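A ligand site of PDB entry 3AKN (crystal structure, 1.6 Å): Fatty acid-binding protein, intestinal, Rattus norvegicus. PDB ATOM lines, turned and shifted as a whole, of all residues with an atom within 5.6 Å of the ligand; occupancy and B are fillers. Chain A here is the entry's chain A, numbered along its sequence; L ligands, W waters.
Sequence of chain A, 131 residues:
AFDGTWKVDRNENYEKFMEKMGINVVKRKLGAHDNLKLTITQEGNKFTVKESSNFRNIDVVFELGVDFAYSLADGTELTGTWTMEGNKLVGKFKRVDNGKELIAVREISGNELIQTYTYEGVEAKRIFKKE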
ATOM      1  N   TYR A  14      -6.586 -18.502   4.543  1.00  0.00           N
ATOM      2  CA  TYR A  14      -6.937 -19.612   5.427  1.00  0.00           C
ATOM      3  C   TYR A  14      -7.817 -20.649   4.751  1.00  0.00           C
ATOM      4  O   TYR A  14      -7.645 -21.863   4.990  1.00  0.00           O
ATOM      5  CB  TYR A  14      -7.501 -19.060   6.751  1.00  0.00           C
ATOM      6  CG  TYR A  14      -7.729 -20.077   7.824  1.00  0.00           C
ATOM      7  CD1 TYR A  14      -6.778 -21.070   8.075  1.00  0.00           C
ATOM      8  CD2 TYR A  14      -8.886 -20.049   8.594  1.00  0.00           C
ATOM      9  CE1 TYR A  14      -6.985 -22.026   9.085  1.00  0.00           C
ATOM     10  CE2 TYR A  14      -9.093 -20.995   9.603  1.00  0.00           C
ATOM     11  CZ  TYR A  14      -8.155 -21.990   9.836  1.00  0.00           C
ATOM     12  OH  TYR A  14      -8.363 -22.928  10.833  1.00  0.00           O
ATOM     13  N   PHE A  17      -5.544 -22.963   2.797  1.00  0.00           N
ATOM     14  CA  PHE A  17      -4.829 -23.813   3.744  1.00  0.00           C
ATOM     15  C   PHE A  17      -5.728 -24.942   4.225  1.00  0.00           C
ATOM     16  O   PHE A  17      -5.330 -26.122   4.250  1.00  0.00           O
ATOM     17  CB  PHE A  17      -4.305 -22.980   4.918  1.00  0.00           C
ATOM     18  CG  PHE A  17      -3.711 -23.785   6.017  1.00  0.00           C
ATOM     19  CD1 PHE A  17      -2.340 -24.132   5.986  1.00  0.00           C
ATOM     20  CD2 PHE A  17      -4.501 -24.231   7.085  1.00  0.00           C
ATOM     21  CE1 PHE A  17      -1.798 -24.905   7.019  1.00  0.00           C
ATOM     22  CE2 PHE A  17      -3.928 -24.994   8.120  1.00  0.00           C
ATOM     23  CZ  PHE A  17      -2.579 -25.323   8.071  1.00  0.00           C
ATOM     24  N   MET A  18      -6.979 -24.609   4.624  1.00  0.00           N
ATOM     25  CA  MET A  18      -7.883 -25.674   5.056  1.00  0.00           C
ATOM     26  C   MET A  18      -8.157 -26.704   3.971  1.00  0.00           C
ATOM     27  O   MET A  18      -8.236 -27.918   4.229  1.00  0.00           O
ATOM     28  CB  MET A  18      -9.211 -25.090   5.571  1.00  0.00           C
ATOM     29  CG  MET A  18      -9.052 -24.288   6.811  1.00  0.00           C
ATOM     30  SD  MET A  18     -10.612 -23.675   7.491  1.00  0.00           S
ATOM     31  CE  MET A  18     -10.880 -22.232   6.470  1.00  0.00           C
ATOM     32  N   MET A  21      -5.391 -29.058   3.816  1.00  0.00           N
ATOM     33  CA  MET A  21      -5.441 -29.991   4.946  1.00  0.00           C
ATOM     34  C   MET A  21      -6.560 -31.042   4.781  1.00  0.00           C
ATOM     35  O   MET A  21      -6.661 -31.958   5.590  1.00  0.00           O
ATOM     36  CB  MET A  21      -5.669 -29.239   6.259  1.00  0.00           C
ATOM     37  CG  MET A  21      -4.422 -28.599   6.842  1.00  0.00           C
ATOM     38  SD  MET A  21      -3.286 -29.802   7.588  1.00  0.00           S
ATOM     39  CE  MET A  21      -4.187 -30.256   9.090  1.00  0.00           C
ATOM     40  N   ILE A  23      -9.991 -30.342   4.443  1.00  0.00           N
ATOM     41  CA  ILE A  23     -11.254 -29.894   5.014  1.00  0.00           C
ATOM     42  C   ILE A  23     -12.269 -29.624   3.895  1.00  0.00           C
ATOM     43  O   ILE A  23     -11.956 -28.938   2.931  1.00  0.00           O
ATOM     44  CB  ILE A  23     -11.047 -28.637   5.898  1.00  0.00           C
ATOM     45  CG1 ILE A  23      -9.931 -28.849   6.948  1.00  0.00           C
ATOM     46  CG2 ILE A  23     -12.360 -28.240   6.598  1.00  0.00           C
ATOM     47  CD1 ILE A  23     -10.040 -30.137   7.766  1.00  0.00           C
ATOM     48  N   LYS A  27     -17.125 -27.105   6.138  1.00  0.00           N
ATOM     49  CA  LYS A  27     -16.277 -26.906   7.322  1.00  0.00           C
ATOM     50  C   LYS A  27     -15.263 -25.781   7.127  1.00  0.00           C
ATOM     51  O   LYS A  27     -14.847 -25.153   8.113  1.00  0.00           O
ATOM     52  CB  LYS A  27     -15.603 -28.209   7.760  1.00  0.00           C
ATOM     53  CG  LYS A  27     -16.538 -29.298   8.305  1.00  0.00           C
ATOM     54  CD  LYS A  27     -17.514 -28.774   9.344  1.00  0.00           C
ATOM     55  CE  LYS A  27     -18.230 -29.913  10.088  1.00  0.00           C
ATOM     56  NZ  LYS A  27     -19.613 -29.568  10.542  1.00  0.00           N
ATOM     57  N   ARG A  28     -14.826 -25.551   5.879  1.00  0.00           N
ATOM     58  CA  ARG A  28     -13.949 -24.394   5.595  1.00  0.00           C
ATOM     59  C   ARG A  28     -14.667 -23.100   5.895  1.00  0.00           C
ATOM     60  O   ARG A  28     -14.129 -22.209   6.535  1.00  0.00           O
ATOM     61  CB  ARG A  28     -13.407 -24.385   4.160  1.00  0.00           C
ATOM     62  CG  ARG A  28     -12.590 -25.625   3.833  1.00  0.00           C
ATOM     63  CD  ARG A  28     -11.726 -25.382   2.623  1.00  0.00           C
ATOM     64  NE  ARG A  28     -12.494 -25.113   1.403  1.00  0.00           N
ATOM     65  CZ  ARG A  28     -12.869 -26.033   0.509  1.00  0.00           C
ATOM     66  NH1 ARG A  28     -12.576 -27.324   0.652  1.00  0.00           N
ATOM     67  NH2 ARG A  28     -13.540 -25.626  -0.563  1.00  0.00           N
ATOM     68  N   GLY A  31     -14.889 -22.779   9.505  1.00  0.00           N
ATOM     69  CA  GLY A  31     -13.555 -22.509  10.058  1.00  0.00           C
ATOM     70  C   GLY A  31     -13.109 -21.068   9.842  1.00  0.00           C
ATOM     71  O   GLY A  31     -12.370 -20.541  10.675  1.00  0.00           O
ATOM     72  N   LEU A  38      -7.581 -17.067  21.902  1.00  0.00           N
ATOM     73  CA  LEU A  38      -6.500 -17.726  22.628  1.00  0.00           C
ATOM     74  C   LEU A  38      -6.177 -16.937  23.879  1.00  0.00           C
ATOM     75  O   LEU A  38      -5.854 -15.738  23.780  1.00  0.00           O
ATOM     76  CB  LEU A  38      -5.228 -17.788  21.778  1.00  0.00           C
ATOM     77  CG  LEU A  38      -5.324 -18.441  20.392  1.00  0.00           C
ATOM     78  CD1 LEU A  38      -4.013 -18.179  19.708  1.00  0.00           C
ATOM     79  CD2 LEU A  38      -5.540 -19.947  20.551  1.00  0.00           C
ATOM     80  N   VAL A  49      -2.359 -22.383  27.088  1.00  0.00           N
ATOM     81  CA  VAL A  49      -3.158 -21.702  26.067  1.00  0.00           C
ATOM     82  C   VAL A  49      -4.573 -22.231  26.180  1.00  0.00           C
ATOM     83  O   VAL A  49      -4.800 -23.434  25.982  1.00  0.00           O
ATOM     84  CB  VAL A  49      -2.619 -21.955  24.637  1.00  0.00           C
ATOM     85  CG1 VAL A  49      -3.474 -21.210  23.629  1.00  0.00           C
ATOM     86  CG2 VAL A  49      -1.156 -21.507  24.535  1.00  0.00           C
ATOM     87  N   GLU A  51      -7.734 -22.504  24.334  1.00  0.00           N
ATOM     88  CA  GLU A  51      -8.241 -22.364  22.967  1.00  0.00           C
ATOM     89  C   GLU A  51      -9.768 -22.417  22.998  1.00  0.00           C
ATOM     90  O   GLU A  51     -10.336 -23.408  23.457  1.00  0.00           O
ATOM     91  CB  GLU A  51      -7.684 -23.489  22.100  1.00  0.00           C
ATOM     92  CG  GLU A  51      -8.307 -23.598  20.737  1.00  0.00           C
ATOM     93  CD  GLU A  51      -7.682 -24.711  19.896  1.00  0.00           C
ATOM     94  OE1 GLU A  51      -6.484 -25.038  20.124  1.00  0.00           O
ATOM     95  OE2 GLU A  51      -8.399 -25.245  19.019  1.00  0.00           O
ATOM     96  N   PHE A  55     -15.737 -24.572  17.443  1.00  0.00           N
ATOM     97  CA  PHE A  55     -15.561 -26.015  17.341  1.00  0.00           C
ATOM     98  C   PHE A  55     -15.350 -26.644  18.687  1.00  0.00           C
ATOM     99  O   PHE A  55     -15.826 -27.759  18.918  1.00  0.00           O
ATOM    100  CB  PHE A  55     -14.402 -26.387  16.421  1.00  0.00           C
ATOM    101  CG  PHE A  55     -14.582 -25.908  15.016  1.00  0.00           C
ATOM    102  CD1 PHE A  55     -15.720 -26.259  14.280  1.00  0.00           C
ATOM    103  CD2 PHE A  55     -13.636 -25.095  14.444  1.00  0.00           C
ATOM    104  CE1 PHE A  55     -15.880 -25.786  12.985  1.00  0.00           C
ATOM    105  CE2 PHE A  55     -13.798 -24.614  13.138  1.00  0.00           C
ATOM    106  CZ  PHE A  55     -14.895 -24.965  12.405  1.00  0.00           C
ATOM    107  N   VAL A  60      -4.636 -26.124  26.500  1.00  0.00           N
ATOM    108  CA  VAL A  60      -3.365 -26.706  26.058  1.00  0.00           C
ATOM    109  C   VAL A  60      -2.290 -26.281  27.032  1.00  0.00           C
ATOM    110  O   VAL A  60      -2.206 -25.112  27.396  1.00  0.00           O
ATOM    111  CB  VAL A  60      -2.984 -26.194  24.650  1.00  0.00           C
ATOM    112  CG1 VAL A  60      -1.659 -26.802  24.180  1.00  0.00           C
ATOM    113  CG2 VAL A  60      -4.097 -26.480  23.654  1.00  0.00           C
ATOM    114  N   PHE A  62       1.980 -26.667  27.400  1.00  0.00           N
ATOM    115  CA  PHE A  62       3.228 -27.157  26.816  1.00  0.00           C
ATOM    116  C   PHE A  62       4.417 -26.449  27.444  1.00  0.00           C
ATOM    117  O   PHE A  62       4.308 -25.350  27.999  1.00  0.00           O
ATOM    118  CB  PHE A  62       3.238 -27.016  25.274  1.00  0.00           C
ATOM    119  CG  PHE A  62       3.189 -25.610  24.770  1.00  0.00           C
ATOM    120  CD1 PHE A  62       4.351 -24.851  24.656  1.00  0.00           C
ATOM    121  CD2 PHE A  62       1.975 -25.048  24.340  1.00  0.00           C
ATOM    122  CE1 PHE A  62       4.311 -23.543  24.173  1.00  0.00           C
ATOM    123  CE2 PHE A  62       1.952 -23.762  23.846  1.00  0.00           C
ATOM    124  CZ  PHE A  62       3.109 -23.000  23.754  1.00  0.00           C
ATOM    125  N   PHE A  68       4.743 -32.792  22.653  1.00  0.00           N
ATOM    126  CA  PHE A  68       3.428 -33.100  23.222  1.00  0.00           C
ATOM    127  C   PHE A  68       2.466 -33.461  22.082  1.00  0.00           C
ATOM    128  O   PHE A  68       2.784 -33.219  20.898  1.00  0.00           O
ATOM    129  CB  PHE A  68       2.922 -31.937  24.083  1.00  0.00           C
ATOM    130  CG  PHE A  68       2.523 -30.711  23.292  1.00  0.00           C
ATOM    131  CD1 PHE A  68       3.487 -29.837  22.801  1.00  0.00           C
ATOM    132  CD2 PHE A  68       1.169 -30.421  23.059  1.00  0.00           C
ATOM    133  CE1 PHE A  68       3.159 -28.714  22.091  1.00  0.00           C
ATOM    134  CE2 PHE A  68       0.812 -29.286  22.353  1.00  0.00           C
ATOM    135  CZ  PHE A  68       1.813 -28.425  21.846  1.00  0.00           C
ATOM    136  N   TYR A  70      -1.464 -33.227  20.383  1.00  0.00           N
ATOM    137  CA  TYR A  70      -2.512 -32.233  20.264  1.00  0.00           C
ATOM    138  C   TYR A  70      -3.457 -32.687  19.185  1.00  0.00           C
ATOM    139  O   TYR A  70      -3.011 -33.100  18.113  1.00  0.00           O
ATOM    140  CB  TYR A  70      -1.912 -30.891  19.866  1.00  0.00           C
ATOM    141  CG  TYR A  70      -2.880 -29.812  19.504  1.00  0.00           C
ATOM    142  CD1 TYR A  70      -3.421 -28.975  20.488  1.00  0.00           C
ATOM    143  CD2 TYR A  70      -3.210 -29.561  18.180  1.00  0.00           C
ATOM    144  CE1 TYR A  70      -4.316 -27.955  20.150  1.00  0.00           C
ATOM    145  CE2 TYR A  70      -4.056 -28.534  17.832  1.00  0.00           C
ATOM    146  CZ  TYR A  70      -4.619 -27.726  18.813  1.00  0.00           C
ATOM    147  OH  TYR A  70      -5.473 -26.707  18.478  1.00  0.00           O
ATOM    148  N   LEU A  72      -6.635 -31.895  16.564  1.00  0.00           N
ATOM    149  CA  LEU A  72      -7.313 -30.822  15.848  1.00  0.00           C
ATOM    150  C   LEU A  72      -8.824 -30.990  15.995  1.00  0.00           C
ATOM    151  O   LEU A  72      -9.270 -31.990  16.564  1.00  0.00           O
ATOM    152  CB  LEU A  72      -6.923 -30.864  14.379  1.00  0.00           C
ATOM    153  CG  LEU A  72      -5.443 -30.566  14.139  1.00  0.00           C
ATOM    154  CD1 LEU A  72      -5.074 -30.935  12.706  1.00  0.00           C
ATOM    155  CD2 LEU A  72      -5.165 -29.098  14.374  1.00  0.00           C
ATOM    156  N   ALA A  73      -9.598 -30.052  15.459  1.00  0.00           N
ATOM    157  CA  ALA A  73     -11.060 -30.008  15.691  1.00  0.00           C
ATOM    158  C   ALA A  73     -11.826 -31.227  15.181  1.00  0.00           C
ATOM    159  O   ALA A  73     -12.972 -31.469  15.604  1.00  0.00           O
ATOM    160  CB  ALA A  73     -11.627 -28.742  15.082  1.00  0.00           C
ATOM    161  N   ASP A  74     -11.227 -31.986  14.268  1.00  0.00           N
ATOM    162  CA  ASP A  74     -11.874 -33.172  13.730  1.00  0.00           C
ATOM    163  C   ASP A  74     -11.255 -34.471  14.251  1.00  0.00           C
ATOM    164  O   ASP A  74     -11.564 -35.552  13.746  1.00  0.00           O
ATOM    165  CB  ASP A  74     -11.839 -33.151  12.199  1.00  0.00           C
ATOM    166  CG  ASP A  74     -10.419 -33.247  11.653  1.00  0.00           C
ATOM    167  OD1 ASP A  74      -9.466 -33.327  12.451  1.00  0.00           O
ATOM    168  OD2 ASP A  74     -10.259 -33.251  10.409  1.00  0.00           O
ATOM    169  N   THR A  76      -7.996 -35.176  14.223  1.00  0.00           N
ATOM    170  CA  THR A  76      -6.692 -35.411  13.595  1.00  0.00           C
ATOM    171  C   THR A  76      -5.613 -35.081  14.613  1.00  0.00           C
ATOM    172  O   THR A  76      -5.570 -33.967  15.157  1.00  0.00           O
ATOM    173  CB  THR A  76      -6.512 -34.517  12.352  1.00  0.00           C
ATOM    174  OG1 THR A  76      -7.485 -34.896  11.372  1.00  0.00           O
ATOM    175  CG2 THR A  76      -5.127 -34.687  11.700  1.00  0.00           C
ATOM    176  N   LEU A  78      -1.857 -34.469  16.112  1.00  0.00           N
ATOM    177  CA  LEU A  78      -0.504 -33.988  15.853  1.00  0.00           C
ATOM    178  C   LEU A  78       0.405 -34.299  17.019  1.00  0.00           C
ATOM    179  O   LEU A  78      -0.053 -34.370  18.167  1.00  0.00           O
ATOM    180  CB  LEU A  78      -0.506 -32.488  15.676  1.00  0.00           C
ATOM    181  CG  LEU A  78      -1.506 -31.821  14.728  1.00  0.00           C
ATOM    182  CD1 LEU A  78      -1.270 -30.330  14.680  1.00  0.00           C
ATOM    183  CD2 LEU A  78      -1.376 -32.449  13.345  1.00  0.00           C
ATOM    184  N   TRP A  82       6.845 -26.694  20.520  1.00  0.00           N
ATOM    185  CA  TRP A  82       7.051 -25.255  20.382  1.00  0.00           C
ATOM    186  C   TRP A  82       8.444 -24.930  20.906  1.00  0.00           C
ATOM    187  O   TRP A  82       8.837 -25.465  21.947  1.00  0.00           O
ATOM    188  CB  TRP A  82       6.053 -24.463  21.226  1.00  0.00           C
ATOM    189  CG  TRP A  82       4.659 -24.405  20.692  1.00  0.00           C
ATOM    190  CD1 TRP A  82       3.581 -25.122  21.123  1.00  0.00           C
ATOM    191  CD2 TRP A  82       4.171 -23.555  19.649  1.00  0.00           C
ATOM    192  NE1 TRP A  82       2.454 -24.774  20.406  1.00  0.00           N
ATOM    193  CE2 TRP A  82       2.792 -23.819  19.494  1.00  0.00           C
ATOM    194  CE3 TRP A  82       4.771 -22.594  18.828  1.00  0.00           C
ATOM    195  CZ2 TRP A  82       2.007 -23.138  18.552  1.00  0.00           C
ATOM    196  CZ3 TRP A  82       3.985 -21.925  17.878  1.00  0.00           C
ATOM    197  CH2 TRP A  82       2.620 -22.215  17.755  1.00  0.00           C
ATOM    198  N   PHE A  93       5.196 -29.416  14.102  1.00  0.00           N
ATOM    199  CA  PHE A  93       4.285 -30.553  14.308  1.00  0.00           C
ATOM    200  C   PHE A  93       4.275 -31.491  13.139  1.00  0.00           C
ATOM    201  O   PHE A  93       4.721 -31.157  12.061  1.00  0.00           O
ATOM    202  CB  PHE A  93       2.863 -30.055  14.617  1.00  0.00           C
ATOM    203  CG  PHE A  93       2.806 -29.238  15.847  1.00  0.00           C
ATOM    204  CD1 PHE A  93       2.992 -27.849  15.781  1.00  0.00           C
ATOM    205  CD2 PHE A  93       2.611 -29.850  17.086  1.00  0.00           C
ATOM    206  CE1 PHE A  93       2.993 -27.092  16.956  1.00  0.00           C
ATOM    207  CE2 PHE A  93       2.613 -29.091  18.271  1.00  0.00           C
ATOM    208  CZ  PHE A  93       2.804 -27.716  18.175  1.00  0.00           C
ATOM    209  N   LEU A 102       3.332 -29.968   9.836  1.00  0.00           N
ATOM    210  CA  LEU A 102       2.446 -28.809   9.931  1.00  0.00           C
ATOM    211  C   LEU A 102       3.197 -27.863  10.870  1.00  0.00           C
ATOM    212  O   LEU A 102       3.539 -28.247  11.973  1.00  0.00           O
ATOM    213  CB  LEU A 102       1.082 -29.210  10.541  1.00  0.00           C
ATOM    214  CG  LEU A 102      -0.017 -28.133  10.504  1.00  0.00           C
ATOM    215  CD1 LEU A 102      -1.358 -28.686  10.904  1.00  0.00           C
ATOM    216  CD2 LEU A 102       0.288 -26.943  11.438  1.00  0.00           C
ATOM    217  N   ALA A 104       3.407 -24.070  12.796  1.00  0.00           N
ATOM    218  CA  ALA A 104       2.752 -22.841  13.227  1.00  0.00           C
ATOM    219  C   ALA A 104       3.806 -21.907  13.779  1.00  0.00           C
ATOM    220  O   ALA A 104       4.718 -22.344  14.468  1.00  0.00           O
ATOM    221  CB  ALA A 104       1.657 -23.106  14.300  1.00  0.00           C
ATOM    222  N   ARG A 106       4.196 -18.149  15.859  1.00  0.00           N
ATOM    223  CA  ARG A 106       3.518 -17.048  16.527  1.00  0.00           C
ATOM    224  C   ARG A 106       4.471 -15.880  16.698  1.00  0.00           C
ATOM    225  O   ARG A 106       5.593 -16.049  17.177  1.00  0.00           O
ATOM    226  CB  ARG A 106       2.989 -17.481  17.891  1.00  0.00           C
ATOM    227  CG  ARG A 106       1.821 -18.434  17.764  1.00  0.00           C
ATOM    228  CD  ARG A 106       1.395 -19.003  19.116  1.00  0.00           C
ATOM    229  NE  ARG A 106       0.102 -19.679  18.998  1.00  0.00           N
ATOM    230  CZ  ARG A 106      -0.326 -20.661  19.767  1.00  0.00           C
ATOM    231  NH1 ARG A 106       0.409 -21.131  20.763  1.00  0.00           N
ATOM    232  NH2 ARG A 106      -1.536 -21.189  19.562  1.00  0.00           N
ATOM    233  N   TYR A 117       0.477 -20.477   9.593  1.00  0.00           N
ATOM    234  CA  TYR A 117       0.545 -21.928   9.411  1.00  0.00           C
ATOM    235  C   TYR A 117       1.208 -22.227   8.106  1.00  0.00           C
ATOM    236  O   TYR A 117       1.014 -21.486   7.143  1.00  0.00           O
ATOM    237  CB  TYR A 117      -0.852 -22.536   9.316  1.00  0.00           C
ATOM    238  CG  TYR A 117      -1.772 -22.292  10.462  1.00  0.00           C
ATOM    239  CD1 TYR A 117      -1.314 -22.322  11.805  1.00  0.00           C
ATOM    240  CD2 TYR A 117      -3.131 -22.063  10.218  1.00  0.00           C
ATOM    241  CE1 TYR A 117      -2.201 -22.110  12.867  1.00  0.00           C
ATOM    242  CE2 TYR A 117      -4.028 -21.851  11.283  1.00  0.00           C
ATOM    243  CZ  TYR A 117      -3.558 -21.878  12.581  1.00  0.00           C
ATOM    244  OH  TYR A 117      -4.428 -21.698  13.634  1.00  0.00           O
HETATM  245  C1  LIG L   1     -10.074 -29.828  11.402  1.00  0.00           C
HETATM  246  C2  LIG L   1     -10.536 -28.581  10.969  1.00  0.00           C
HETATM  247  C3  LIG L   1      -9.602 -27.551  10.433  1.00  0.00           C
HETATM  248  C4  LIG L   1      -8.142 -27.893  10.385  1.00  0.00           C
HETATM  249  C5  LIG L   1      -7.793 -29.186  10.825  1.00  0.00           C
HETATM  250  C6  LIG L   1      -8.719 -30.102  11.314  1.00  0.00           C
HETATM  251  C7  LIG L   1     -11.968 -28.216  11.051  1.00  0.00           C
HETATM  252  C8  LIG L   1     -12.367 -26.967  10.575  1.00  0.00           C
HETATM  253  C9  LIG L   1     -11.443 -26.032  10.073  1.00  0.00           C
HETATM  254  C10 LIG L   1     -10.075 -26.314  10.004  1.00  0.00           C
HETATM  255  N1  LIG L   1     -12.983 -29.092  11.439  1.00  0.00           N
HETATM  256  C11 LIG L   1     -13.146 -30.304  10.665  1.00  0.00           C
HETATM  257  C12 LIG L   1     -14.051 -28.742  12.365  1.00  0.00           C
HETATM  258  S1  LIG L   1      -7.032 -26.873   9.815  1.00  0.00           S
HETATM  259  O1  LIG L   1      -7.354 -26.440   8.485  1.00  0.00           O
HETATM  260  O2  LIG L   1      -5.746 -27.514   9.901  1.00  0.00           O
HETATM  261  N2  LIG L   1      -6.921 -25.593  10.775  1.00  0.00           N
HETATM  262  C13 LIG L   1      -6.432 -25.712  12.144  1.00  0.00           C
HETATM  263  C14 LIG L   1      -4.917 -25.522  12.230  1.00  0.00           C
HETATM  264  C15 LIG L   1      -4.450 -25.569  13.675  1.00  0.00           C
HETATM  265  C16 LIG L   1      -2.939 -25.749  13.790  1.00  0.00           C
HETATM  266  C17 LIG L   1      -2.574 -25.766  15.283  1.00  0.00           C
HETATM  267  C18 LIG L   1      -1.070 -25.663  15.547  1.00  0.00           C
HETATM  268  C19 LIG L   1      -0.676 -26.363  16.856  1.00  0.00           C
HETATM  269  C20 LIG L   1      -1.279 -25.709  18.102  1.00  0.00           C
HETATM  270  C21 LIG L   1      -0.686 -26.331  19.362  1.00  0.00           C
HETATM  271  C22 LIG L   1      -1.308 -25.793  20.648  1.00  0.00           C
HETATM  272  C23 LIG L   1      -1.072 -24.315  20.869  1.00  0.00           C
HETATM  273  O3  LIG L   1       0.097 -23.926  21.008  1.00  0.00           O
HETATM  274  O4  LIG L   1      -2.041 -23.515  20.904  1.00  0.00           O
HETATM  275  O   HOH W   1     -10.178 -25.579  13.422  1.00  0.00           O
HETATM  276  O   HOH W   2     -12.720 -32.997   8.653  1.00  0.00           O
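An oxygen (O4) of the ligand lies within salt-bridge range of the guanidinium group (NH2) of Arg 106, 2.7 Å away. A nitrogen (N2) of the ligand sits at hydrogen-bond distance from the side-chain hydroxyl of Tyr 14 (3.0 Å). NE1 of Trp 82 lies within hydrogen-bond range of O3 of the ligand (2.6 Å).
The side-chain carboxylate of Asp 74 sits at hydrogen-bond distance from the side-chain hydroxyl of Thr 76. The backbone carbonyl oxygen of Phe 93 is in hydrogen-bond range of the backbone NH of Leu 102, at 2.9 Å. The backbone carbonyl oxygen (O) of Met 18 is in hydrogen-bond range of the backbone NH (N) of Ile 23. The side-chain hydroxyl (OH) of Tyr 70 is in hydrogen-bond range of the side-chain carboxylate (OE1) of Glu 51 (2.6 Å). O of Tyr 70 lies within hydrogen-bond range of N of Leu 78. The backbone carbonyl oxygen of Val 49 is in hydrogen-bond range of the backbone NH of Val 60. O of Ile 23 sits at hydrogen-bond distance from NH1 of Arg 28, at 2.9 Å.
Phe 17 touches the ligand. CG of Met 18 touches O1 of the ligand (3.2 Å). Met 21 touches the ligand (CE to O2, 3.3 Å). Ile 23 touches the ligand (CD1 to C2, 3.6 Å). O of Lys 27 touches C8 of the ligand, at 3.9 Å. Val 49 touches the ligand. Phe 55 touches the ligand. Val 60 touches the ligand (CG1 to C22, 3.7 Å). CE2 of Phe 62 touches O3 of the ligand, 3.4 Å away. Tyr 70 touches the ligand. Leu 72 touches the ligand. Ala 73 touches the ligand. Asp 74 touches the ligand. Phe 93 touches the ligand. Ala 104 touches the ligand. CE1 of Tyr 117 touches C16 of the ligand, 3.8 Å away. Hydrophobic or aromatic side chains that line the ligand: Tyr 14, Phe 17, Met 18, Met 21, Ile 23, Val 49, Phe 55, Val 60, Phe 62, Tyr 70, Leu 72, Ala 73, Trp 82, Phe 93, Ala 104 and Tyr 117. The nearest printed residue that does not touch the ligand is Phe 68 (4.1 Å).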
